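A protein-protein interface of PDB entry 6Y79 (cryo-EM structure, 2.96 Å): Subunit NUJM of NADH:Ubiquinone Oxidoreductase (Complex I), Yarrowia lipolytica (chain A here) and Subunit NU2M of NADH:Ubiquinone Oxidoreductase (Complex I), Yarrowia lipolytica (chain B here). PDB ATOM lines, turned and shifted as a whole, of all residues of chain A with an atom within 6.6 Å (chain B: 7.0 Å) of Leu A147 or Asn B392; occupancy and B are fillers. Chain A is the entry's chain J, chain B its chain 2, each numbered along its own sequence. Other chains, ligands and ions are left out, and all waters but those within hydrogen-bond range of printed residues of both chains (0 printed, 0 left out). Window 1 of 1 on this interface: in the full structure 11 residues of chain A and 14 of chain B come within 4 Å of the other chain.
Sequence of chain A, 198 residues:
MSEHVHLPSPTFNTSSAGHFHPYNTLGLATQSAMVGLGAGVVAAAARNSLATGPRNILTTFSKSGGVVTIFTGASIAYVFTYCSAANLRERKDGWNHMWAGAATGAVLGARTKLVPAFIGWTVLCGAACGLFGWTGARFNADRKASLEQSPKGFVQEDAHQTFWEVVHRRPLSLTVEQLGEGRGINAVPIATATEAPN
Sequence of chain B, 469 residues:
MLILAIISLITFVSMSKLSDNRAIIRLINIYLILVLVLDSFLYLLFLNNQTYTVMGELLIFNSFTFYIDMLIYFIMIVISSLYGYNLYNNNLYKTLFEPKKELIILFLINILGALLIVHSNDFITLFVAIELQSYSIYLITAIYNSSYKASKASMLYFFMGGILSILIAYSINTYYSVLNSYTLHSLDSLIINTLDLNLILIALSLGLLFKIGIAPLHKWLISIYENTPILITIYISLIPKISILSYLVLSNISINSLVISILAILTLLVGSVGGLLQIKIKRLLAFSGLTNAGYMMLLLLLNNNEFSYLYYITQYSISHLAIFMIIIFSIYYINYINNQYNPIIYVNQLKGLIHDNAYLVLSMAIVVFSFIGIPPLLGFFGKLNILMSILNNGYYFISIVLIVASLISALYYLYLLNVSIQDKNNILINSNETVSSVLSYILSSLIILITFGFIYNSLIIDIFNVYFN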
ATOM      1  N   ASP A 142       6.776   1.658  17.802  1.00  0.00           N
ATOM      2  CA  ASP A 142       6.485   2.411  16.598  1.00  0.00           C
ATOM      3  C   ASP A 142       5.331   1.721  15.886  1.00  0.00           C
ATOM      4  O   ASP A 142       5.234   0.493  15.880  1.00  0.00           O
ATOM      5  CB  ASP A 142       7.715   2.482  15.694  1.00  0.00           C
ATOM      6  CG  ASP A 142       7.576   3.503  14.588  1.00  0.00           C
ATOM      7  OD1 ASP A 142       6.552   4.211  14.541  1.00  0.00           O
ATOM      8  OD2 ASP A 142       8.500   3.598  13.758  1.00  0.00           O
ATOM      9  N   ARG A 143       4.449   2.519  15.298  1.00  0.00           N
ATOM     10  CA  ARG A 143       3.190   1.979  14.801  1.00  0.00           C
ATOM     11  C   ARG A 143       3.356   1.318  13.444  1.00  0.00           C
ATOM     12  O   ARG A 143       3.025   0.143  13.268  1.00  0.00           O
ATOM     13  CB  ARG A 143       2.153   3.096  14.727  1.00  0.00           C
ATOM     14  CG  ARG A 143       1.625   3.491  16.073  1.00  0.00           C
ATOM     15  CD  ARG A 143       1.064   2.279  16.776  1.00  0.00           C
ATOM     16  NE  ARG A 143       0.013   2.667  17.703  1.00  0.00           N
ATOM     17  CZ  ARG A 143      -0.663   1.814  18.454  1.00  0.00           C
ATOM     18  NH1 ARG A 143      -1.604   2.262  19.269  1.00  0.00           N
ATOM     19  NH2 ARG A 143      -0.398   0.519  18.386  1.00  0.00           N
ATOM     20  N   LYS A 144       3.858   2.065  12.468  1.00  0.00           N
ATOM     21  CA  LYS A 144       3.939   1.544  11.114  1.00  0.00           C
ATOM     22  C   LYS A 144       5.138   0.629  10.924  1.00  0.00           C
ATOM     23  O   LYS A 144       5.159  -0.159   9.974  1.00  0.00           O
ATOM     24  CB  LYS A 144       3.992   2.695  10.110  1.00  0.00           C
ATOM     25  CG  LYS A 144       2.631   3.201   9.637  1.00  0.00           C
ATOM     26  CD  LYS A 144       1.955   4.096  10.665  1.00  0.00           C
ATOM     27  CE  LYS A 144       2.714   5.391  10.870  1.00  0.00           C
ATOM     28  NZ  LYS A 144       2.062   6.222  11.912  1.00  0.00           N
ATOM     29  N   ALA A 145       6.132   0.715  11.803  1.00  0.00           N
ATOM     30  CA  ALA A 145       7.281  -0.169  11.739  1.00  0.00           C
ATOM     31  C   ALA A 145       6.990  -1.562  12.275  1.00  0.00           C
ATOM     32  O   ALA A 145       7.794  -2.469  12.047  1.00  0.00           O
ATOM     33  CB  ALA A 145       8.448   0.443  12.511  1.00  0.00           C
ATOM     34  N   SER A 146       5.872  -1.743  12.976  1.00  0.00           N
ATOM     35  CA  SER A 146       5.477  -3.016  13.555  1.00  0.00           C
ATOM     36  C   SER A 146       5.228  -4.045  12.466  1.00  0.00           C
ATOM     37  O   SER A 146       4.992  -3.709  11.315  1.00  0.00           O
ATOM     38  CB  SER A 146       4.202  -2.853  14.369  1.00  0.00           C
ATOM     39  OG  SER A 146       4.356  -1.891  15.384  1.00  0.00           O
ATOM     40  N   LEU A 147       5.278  -5.318  12.837  1.00  0.00           N
ATOM     41  CA  LEU A 147       4.895  -6.343  11.876  1.00  0.00           C
ATOM     42  C   LEU A 147       3.382  -6.377  11.693  1.00  0.00           C
ATOM     43  O   LEU A 147       2.898  -6.698  10.606  1.00  0.00           O
ATOM     44  CB  LEU A 147       5.445  -7.702  12.308  1.00  0.00           C
ATOM     45  CG  LEU A 147       5.029  -8.962  11.552  1.00  0.00           C
ATOM     46  CD1 LEU A 147       5.417  -8.909  10.103  1.00  0.00           C
ATOM     47  CD2 LEU A 147       5.632 -10.161  12.189  1.00  0.00           C
ATOM     48  N   GLU A 148       2.620  -6.002  12.730  1.00  0.00           N
ATOM     49  CA  GLU A 148       1.157  -6.028  12.654  1.00  0.00           C
ATOM     50  C   GLU A 148       0.615  -5.045  11.618  1.00  0.00           C
ATOM     51  O   GLU A 148      -0.420  -5.310  10.998  1.00  0.00           O
ATOM     52  CB  GLU A 148       0.523  -5.726  14.027  1.00  0.00           C
ATOM     53  CG  GLU A 148       0.901  -4.348  14.578  1.00  0.00           C
ATOM     54  CD  GLU A 148       0.033  -3.901  15.712  1.00  0.00           C
ATOM     55  OE1 GLU A 148      -0.845  -4.649  16.168  1.00  0.00           O
ATOM     56  OE2 GLU A 148       0.256  -2.737  16.181  1.00  0.00           O
ATOM     57  N   GLN A 149       1.292  -3.913  11.424  1.00  0.00           N
ATOM     58  CA  GLN A 149       0.792  -2.800  10.636  1.00  0.00           C
ATOM     59  C   GLN A 149       1.647  -2.563   9.403  1.00  0.00           C
ATOM     60  O   GLN A 149       1.679  -1.450   8.869  1.00  0.00           O
ATOM     61  CB  GLN A 149       0.712  -1.537  11.499  1.00  0.00           C
ATOM     62  CG  GLN A 149      -0.407  -1.555  12.555  1.00  0.00           C
ATOM     63  CD  GLN A 149      -0.493  -0.274  13.382  1.00  0.00           C
ATOM     64  OE1 GLN A 149       0.172   0.719  13.092  1.00  0.00           O
ATOM     65  NE2 GLN A 149      -1.309  -0.304  14.430  1.00  0.00           N
ATOM     66  N   SER A 150       2.350  -3.594   8.952  1.00  0.00           N
ATOM     67  CA  SER A 150       3.212  -3.555   7.794  1.00  0.00           C
ATOM     68  C   SER A 150       2.793  -4.617   6.793  1.00  0.00           C
ATOM     69  O   SER A 150       2.116  -5.583   7.153  1.00  0.00           O
ATOM     70  CB  SER A 150       4.676  -3.796   8.169  1.00  0.00           C
ATOM     71  OG  SER A 150       5.140  -2.795   9.051  1.00  0.00           O
ATOM     72  N   PRO A 151       3.161  -4.446   5.525  1.00  0.00           N
ATOM     73  CA  PRO A 151       3.038  -5.545   4.563  1.00  0.00           C
ATOM     74  C   PRO A 151       3.960  -6.701   4.919  1.00  0.00           C
ATOM     75  O   PRO A 151       5.151  -6.519   5.168  1.00  0.00           O
ATOM     76  CB  PRO A 151       3.440  -4.891   3.241  1.00  0.00           C
ATOM     77  CG  PRO A 151       3.189  -3.455   3.442  1.00  0.00           C
ATOM     78  CD  PRO A 151       3.464  -3.166   4.861  1.00  0.00           C
ATOM     79  N   LYS A 152       3.398  -7.901   4.910  1.00  0.00           N
ATOM     80  CA  LYS A 152       4.073  -9.092   5.384  1.00  0.00           C
ATOM     81  C   LYS A 152       3.814 -10.204   4.378  1.00  0.00           C
ATOM     82  O   LYS A 152       3.216  -9.980   3.323  1.00  0.00           O
ATOM     83  CB  LYS A 152       3.574  -9.444   6.790  1.00  0.00           C
ATOM     84  CG  LYS A 152       2.122  -9.888   6.817  1.00  0.00           C
ATOM     85  CD  LYS A 152       1.661 -10.204   8.213  1.00  0.00           C
ATOM     86  CE  LYS A 152       1.276  -8.948   8.944  1.00  0.00           C
ATOM     87  NZ  LYS A 152       0.993  -9.217  10.378  1.00  0.00           N
ATOM     88  N   GLY A 153       4.260 -11.412   4.710  1.00  0.00           N
ATOM     89  CA  GLY A 153       4.002 -12.572   3.888  1.00  0.00           C
ATOM     90  C   GLY A 153       4.790 -12.529   2.594  1.00  0.00           C
ATOM     91  O   GLY A 153       5.767 -11.797   2.447  1.00  0.00           O
ATOM     92  N   TRP A 164      10.115  -7.129   6.358  1.00  0.00           N
ATOM     93  CA  TRP A 164       9.085  -8.059   6.842  1.00  0.00           C
ATOM     94  C   TRP A 164       8.490  -8.935   5.747  1.00  0.00           C
ATOM     95  O   TRP A 164       7.604  -9.742   6.041  1.00  0.00           O
ATOM     96  CB  TRP A 164       7.925  -7.387   7.600  1.00  0.00           C
ATOM     97  CG  TRP A 164       8.286  -6.702   8.868  1.00  0.00           C
ATOM     98  CD1 TRP A 164       8.181  -5.378   9.131  1.00  0.00           C
ATOM     99  CD2 TRP A 164       8.789  -7.308  10.060  1.00  0.00           C
ATOM    100  NE1 TRP A 164       8.600  -5.115  10.406  1.00  0.00           N
ATOM    101  CE2 TRP A 164       8.975  -6.289  10.999  1.00  0.00           C
ATOM    102  CE3 TRP A 164       9.097  -8.615  10.423  1.00  0.00           C
ATOM    103  CZ2 TRP A 164       9.460  -6.535  12.274  1.00  0.00           C
ATOM    104  CZ3 TRP A 164       9.573  -8.857  11.686  1.00  0.00           C
ATOM    105  CH2 TRP A 164       9.751  -7.827  12.595  1.00  0.00           C
ATOM    106  N   LEU B 302      -0.774  -4.170  24.287  1.00  0.00           N
ATOM    107  CA  LEU B 302      -1.034  -4.922  23.079  1.00  0.00           C
ATOM    108  C   LEU B 302      -2.476  -4.766  22.643  1.00  0.00           C
ATOM    109  O   LEU B 302      -3.381  -4.593  23.459  1.00  0.00           O
ATOM    110  CB  LEU B 302      -0.759  -6.406  23.313  1.00  0.00           C
ATOM    111  CG  LEU B 302       0.605  -7.021  23.082  1.00  0.00           C
ATOM    112  CD1 LEU B 302       0.833  -6.781  21.697  1.00  0.00           C
ATOM    113  CD2 LEU B 302       1.690  -6.376  23.861  1.00  0.00           C
ATOM    114  N   ILE B 386       4.165 -14.827  25.067  1.00  0.00           N
ATOM    115  CA  ILE B 386       4.261 -13.403  25.368  1.00  0.00           C
ATOM    116  C   ILE B 386       5.260 -12.734  24.436  1.00  0.00           C
ATOM    117  O   ILE B 386       4.993 -11.652  23.909  1.00  0.00           O
ATOM    118  CB  ILE B 386       4.617 -13.181  26.847  1.00  0.00           C
ATOM    119  CG1 ILE B 386       3.421 -13.489  27.729  1.00  0.00           C
ATOM    120  CG2 ILE B 386       5.035 -11.752  27.116  1.00  0.00           C
ATOM    121  CD1 ILE B 386       3.754 -13.487  29.173  1.00  0.00           C
ATOM    122  N   LEU B 387       6.412 -13.377  24.196  1.00  0.00           N
ATOM    123  CA  LEU B 387       7.419 -12.824  23.287  1.00  0.00           C
ATOM    124  C   LEU B 387       6.906 -12.714  21.858  1.00  0.00           C
ATOM    125  O   LEU B 387       7.243 -11.766  21.145  1.00  0.00           O
ATOM    126  CB  LEU B 387       8.672 -13.690  23.303  1.00  0.00           C
ATOM    127  CG  LEU B 387       9.638 -13.599  24.471  1.00  0.00           C
ATOM    128  CD1 LEU B 387      10.649 -14.720  24.352  1.00  0.00           C
ATOM    129  CD2 LEU B 387      10.318 -12.256  24.469  1.00  0.00           C
ATOM    130  N   MET B 388       6.096 -13.683  21.424  1.00  0.00           N
ATOM    131  CA  MET B 388       5.533 -13.655  20.076  1.00  0.00           C
ATOM    132  C   MET B 388       4.568 -12.502  19.881  1.00  0.00           C
ATOM    133  O   MET B 388       4.349 -12.074  18.751  1.00  0.00           O
ATOM    134  CB  MET B 388       4.818 -14.964  19.766  1.00  0.00           C
ATOM    135  CG  MET B 388       5.723 -16.140  19.562  1.00  0.00           C
ATOM    136  SD  MET B 388       4.799 -17.661  19.366  1.00  0.00           S
ATOM    137  CE  MET B 388       4.234 -17.489  17.681  1.00  0.00           C
ATOM    138  N   SER B 389       3.957 -12.010  20.953  1.00  0.00           N
ATOM    139  CA  SER B 389       3.138 -10.812  20.889  1.00  0.00           C
ATOM    140  C   SER B 389       3.942  -9.548  21.122  1.00  0.00           C
ATOM    141  O   SER B 389       3.573  -8.494  20.630  1.00  0.00           O
ATOM    142  CB  SER B 389       2.015 -10.883  21.921  1.00  0.00           C
ATOM    143  OG  SER B 389       1.141 -11.955  21.648  1.00  0.00           O
ATOM    144  N   ILE B 390       5.009  -9.598  21.898  1.00  0.00           N
ATOM    145  CA  ILE B 390       5.800  -8.394  22.114  1.00  0.00           C
ATOM    146  C   ILE B 390       6.552  -8.017  20.841  1.00  0.00           C
ATOM    147  O   ILE B 390       6.545  -6.857  20.421  1.00  0.00           O
ATOM    148  CB  ILE B 390       6.741  -8.603  23.312  1.00  0.00           C
ATOM    149  CG1 ILE B 390       5.945  -8.644  24.612  1.00  0.00           C
ATOM    150  CG2 ILE B 390       7.731  -7.517  23.410  1.00  0.00           C
ATOM    151  CD1 ILE B 390       5.069  -7.466  24.842  1.00  0.00           C
ATOM    152  N   LEU B 391       7.143  -9.004  20.169  1.00  0.00           N
ATOM    153  CA  LEU B 391       7.959  -8.742  18.992  1.00  0.00           C
ATOM    154  C   LEU B 391       7.130  -8.465  17.748  1.00  0.00           C
ATOM    155  O   LEU B 391       7.592  -7.755  16.849  1.00  0.00           O
ATOM    156  CB  LEU B 391       8.883  -9.927  18.738  1.00  0.00           C
ATOM    157  CG  LEU B 391      10.019 -10.039  19.737  1.00  0.00           C
ATOM    158  CD1 LEU B 391      10.815 -11.286  19.491  1.00  0.00           C
ATOM    159  CD2 LEU B 391      10.879  -8.841  19.573  1.00  0.00           C
ATOM    160  N   ASN B 392       5.920  -9.019  17.678  1.00  0.00           N
ATOM    161  CA  ASN B 392       5.005  -8.763  16.570  1.00  0.00           C
ATOM    162  C   ASN B 392       4.576  -7.306  16.512  1.00  0.00           C
ATOM    163  O   ASN B 392       4.176  -6.813  15.455  1.00  0.00           O
ATOM    164  CB  ASN B 392       3.782  -9.657  16.734  1.00  0.00           C
ATOM    165  CG  ASN B 392       2.925  -9.736  15.511  1.00  0.00           C
ATOM    166  OD1 ASN B 392       3.307  -9.310  14.435  1.00  0.00           O
ATOM    167  ND2 ASN B 392       1.736 -10.294  15.673  1.00  0.00           N
ATOM    168  N   ASN B 393       4.648  -6.603  17.632  1.00  0.00           N
ATOM    169  CA  ASN B 393       3.989  -5.321  17.779  1.00  0.00           C
ATOM    170  C   ASN B 393       4.975  -4.198  18.067  1.00  0.00           C
ATOM    171  O   ASN B 393       4.560  -3.098  18.418  1.00  0.00           O
ATOM    172  CB  ASN B 393       2.922  -5.454  18.864  1.00  0.00           C
ATOM    173  CG  ASN B 393       1.807  -6.452  18.470  1.00  0.00           C
ATOM    174  OD1 ASN B 393       1.953  -7.647  18.599  1.00  0.00           O
ATOM    175  ND2 ASN B 393       0.645  -5.924  18.100  1.00  0.00           N
ATOM    176  N   GLY B 394       6.269  -4.448  17.911  1.00  0.00           N
ATOM    177  CA  GLY B 394       7.263  -3.398  17.876  1.00  0.00           C
ATOM    178  C   GLY B 394       7.924  -3.025  19.181  1.00  0.00           C
ATOM    179  O   GLY B 394       8.549  -1.962  19.250  1.00  0.00           O
ATOM    180  N   TYR B 395       7.813  -3.849  20.213  1.00  0.00           N
ATOM    181  CA  TYR B 395       8.389  -3.525  21.517  1.00  0.00           C
ATOM    182  C   TYR B 395       9.740  -4.217  21.662  1.00  0.00           C
ATOM    183  O   TYR B 395       9.880  -5.274  22.265  1.00  0.00           O
ATOM    184  CB  TYR B 395       7.430  -3.914  22.633  1.00  0.00           C
ATOM    185  CG  TYR B 395       6.131  -3.166  22.582  1.00  0.00           C
ATOM    186  CD1 TYR B 395       6.020  -1.900  23.128  1.00  0.00           C
ATOM    187  CD2 TYR B 395       5.021  -3.721  21.975  1.00  0.00           C
ATOM    188  CE1 TYR B 395       4.836  -1.214  23.072  1.00  0.00           C
ATOM    189  CE2 TYR B 395       3.838  -3.044  21.911  1.00  0.00           C
ATOM    190  CZ  TYR B 395       3.753  -1.791  22.458  1.00  0.00           C
ATOM    191  OH  TYR B 395       2.568  -1.116  22.395  1.00  0.00           O
ATOM    192  N   TYR B 396      10.754  -3.572  21.094  1.00  0.00           N
ATOM    193  CA  TYR B 396      12.049  -4.217  20.946  1.00  0.00           C
ATOM    194  C   TYR B 396      12.935  -4.028  22.163  1.00  0.00           C
ATOM    195  O   TYR B 396      13.630  -4.963  22.560  1.00  0.00           O
ATOM    196  CB  TYR B 396      12.728  -3.705  19.681  1.00  0.00           C
ATOM    197  CG  TYR B 396      11.944  -4.070  18.457  1.00  0.00           C
ATOM    198  CD1 TYR B 396      11.543  -5.379  18.248  1.00  0.00           C
ATOM    199  CD2 TYR B 396      11.572  -3.115  17.531  1.00  0.00           C
ATOM    200  CE1 TYR B 396      10.809  -5.728  17.145  1.00  0.00           C
ATOM    201  CE2 TYR B 396      10.839  -3.453  16.424  1.00  0.00           C
ATOM    202  CZ  TYR B 396      10.461  -4.756  16.235  1.00  0.00           C
ATOM    203  OH  TYR B 396       9.726  -5.082  15.126  1.00  0.00           O
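The backbone carbonyl oxygen (O) of Asn B393 is in hydrogen-bond range of the side-chain hydroxyl (OG) of Ser A146, 3.3 Å away.
The backbone NH (N) of Leu A147 is in hydrogen-bond range of the backbone carbonyl oxygen (O) of Asn B392 (3.2 Å).
The backbone NH of Glu A148 sits at hydrogen-bond distance from the backbone carbonyl oxygen of Asn B392, 3.2 Å away.
The side-chain carboxylate of Glu A148 is in hydrogen-bond range of the side-chain amide nitrogen of Asn B393, at 2.8 Å.
Trp A164 touches Tyr B396.
Of the 12 printed residues of chain B, 3 touch a printed residue of chain A.
Of the 13 printed residues of chain A, 4 touch a printed residue of chain B.
Hydrophobic or aromatic side chains of chain A within 4 Å of the printed part of chain B: Leu A147 and Trp A164.
Along chain A the printed residues that touch a printed residue of chain B span positions 146 to 164.
Among the printed residues, no Asp or Glu carboxylate lies within 4 Å of a Lys or Arg side-chain nitrogen of the other chain.
Leu A147 touches just one residue of chain B: Asn B392 (3.2 Å).
Asn B392 touches just these residues of chain A: Leu A147 and Glu A148.
Of the printed residues of chain B, Trp A164 touches Tyr B396.
Of the printed residues of chain B, Ser A146 touches Asn B393.
Of the printed residues of chain B, Glu A148 touches Asn B392 (3.2 Å) and Asn B393 (2.8 Å).
Of the printed residues of chain A, Tyr B396 touches Trp A164.
Printed residues of chain A within 4 Å of Asn B393: Ser A146 (3.3 Å) and Glu A148 (2.8 Å).
Arg A143 touches none of the printed residues of chain B.
Tyr B395 touches none of the printed residues of chain A.
The nearest residue of chain A that does not touch Asn B392 is Ser A146 (4.1 Å).
The side-chain hydroxyl of Ser A146 is in hydrogen-bond range of the backbone carbonyl oxygen of Asp A142 (2.6 Å).
The backbone carbonyl oxygen (O) of Arg A143 sits at hydrogen-bond distance from the side-chain hydroxyl (OG) of Ser A146.
The guanidinium group (NH2) of Arg A143 lies within salt-bridge range of the side-chain carboxylate (OE2) of Glu A148, 3.99 Å away.
The indole nitrogen of Trp A164 lies within hydrogen-bond range of the backbone carbonyl oxygen of Ala A145, at 3.2 Å.
OE2 of Glu A148 is in hydrogen-bond range of NE2 of Gln A149 (3.4 Å).
The backbone carbonyl oxygen (O) of Ser B389 sits close to the side-chain amide oxygen (OD1) of Asn B393, at 2.7 Å.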
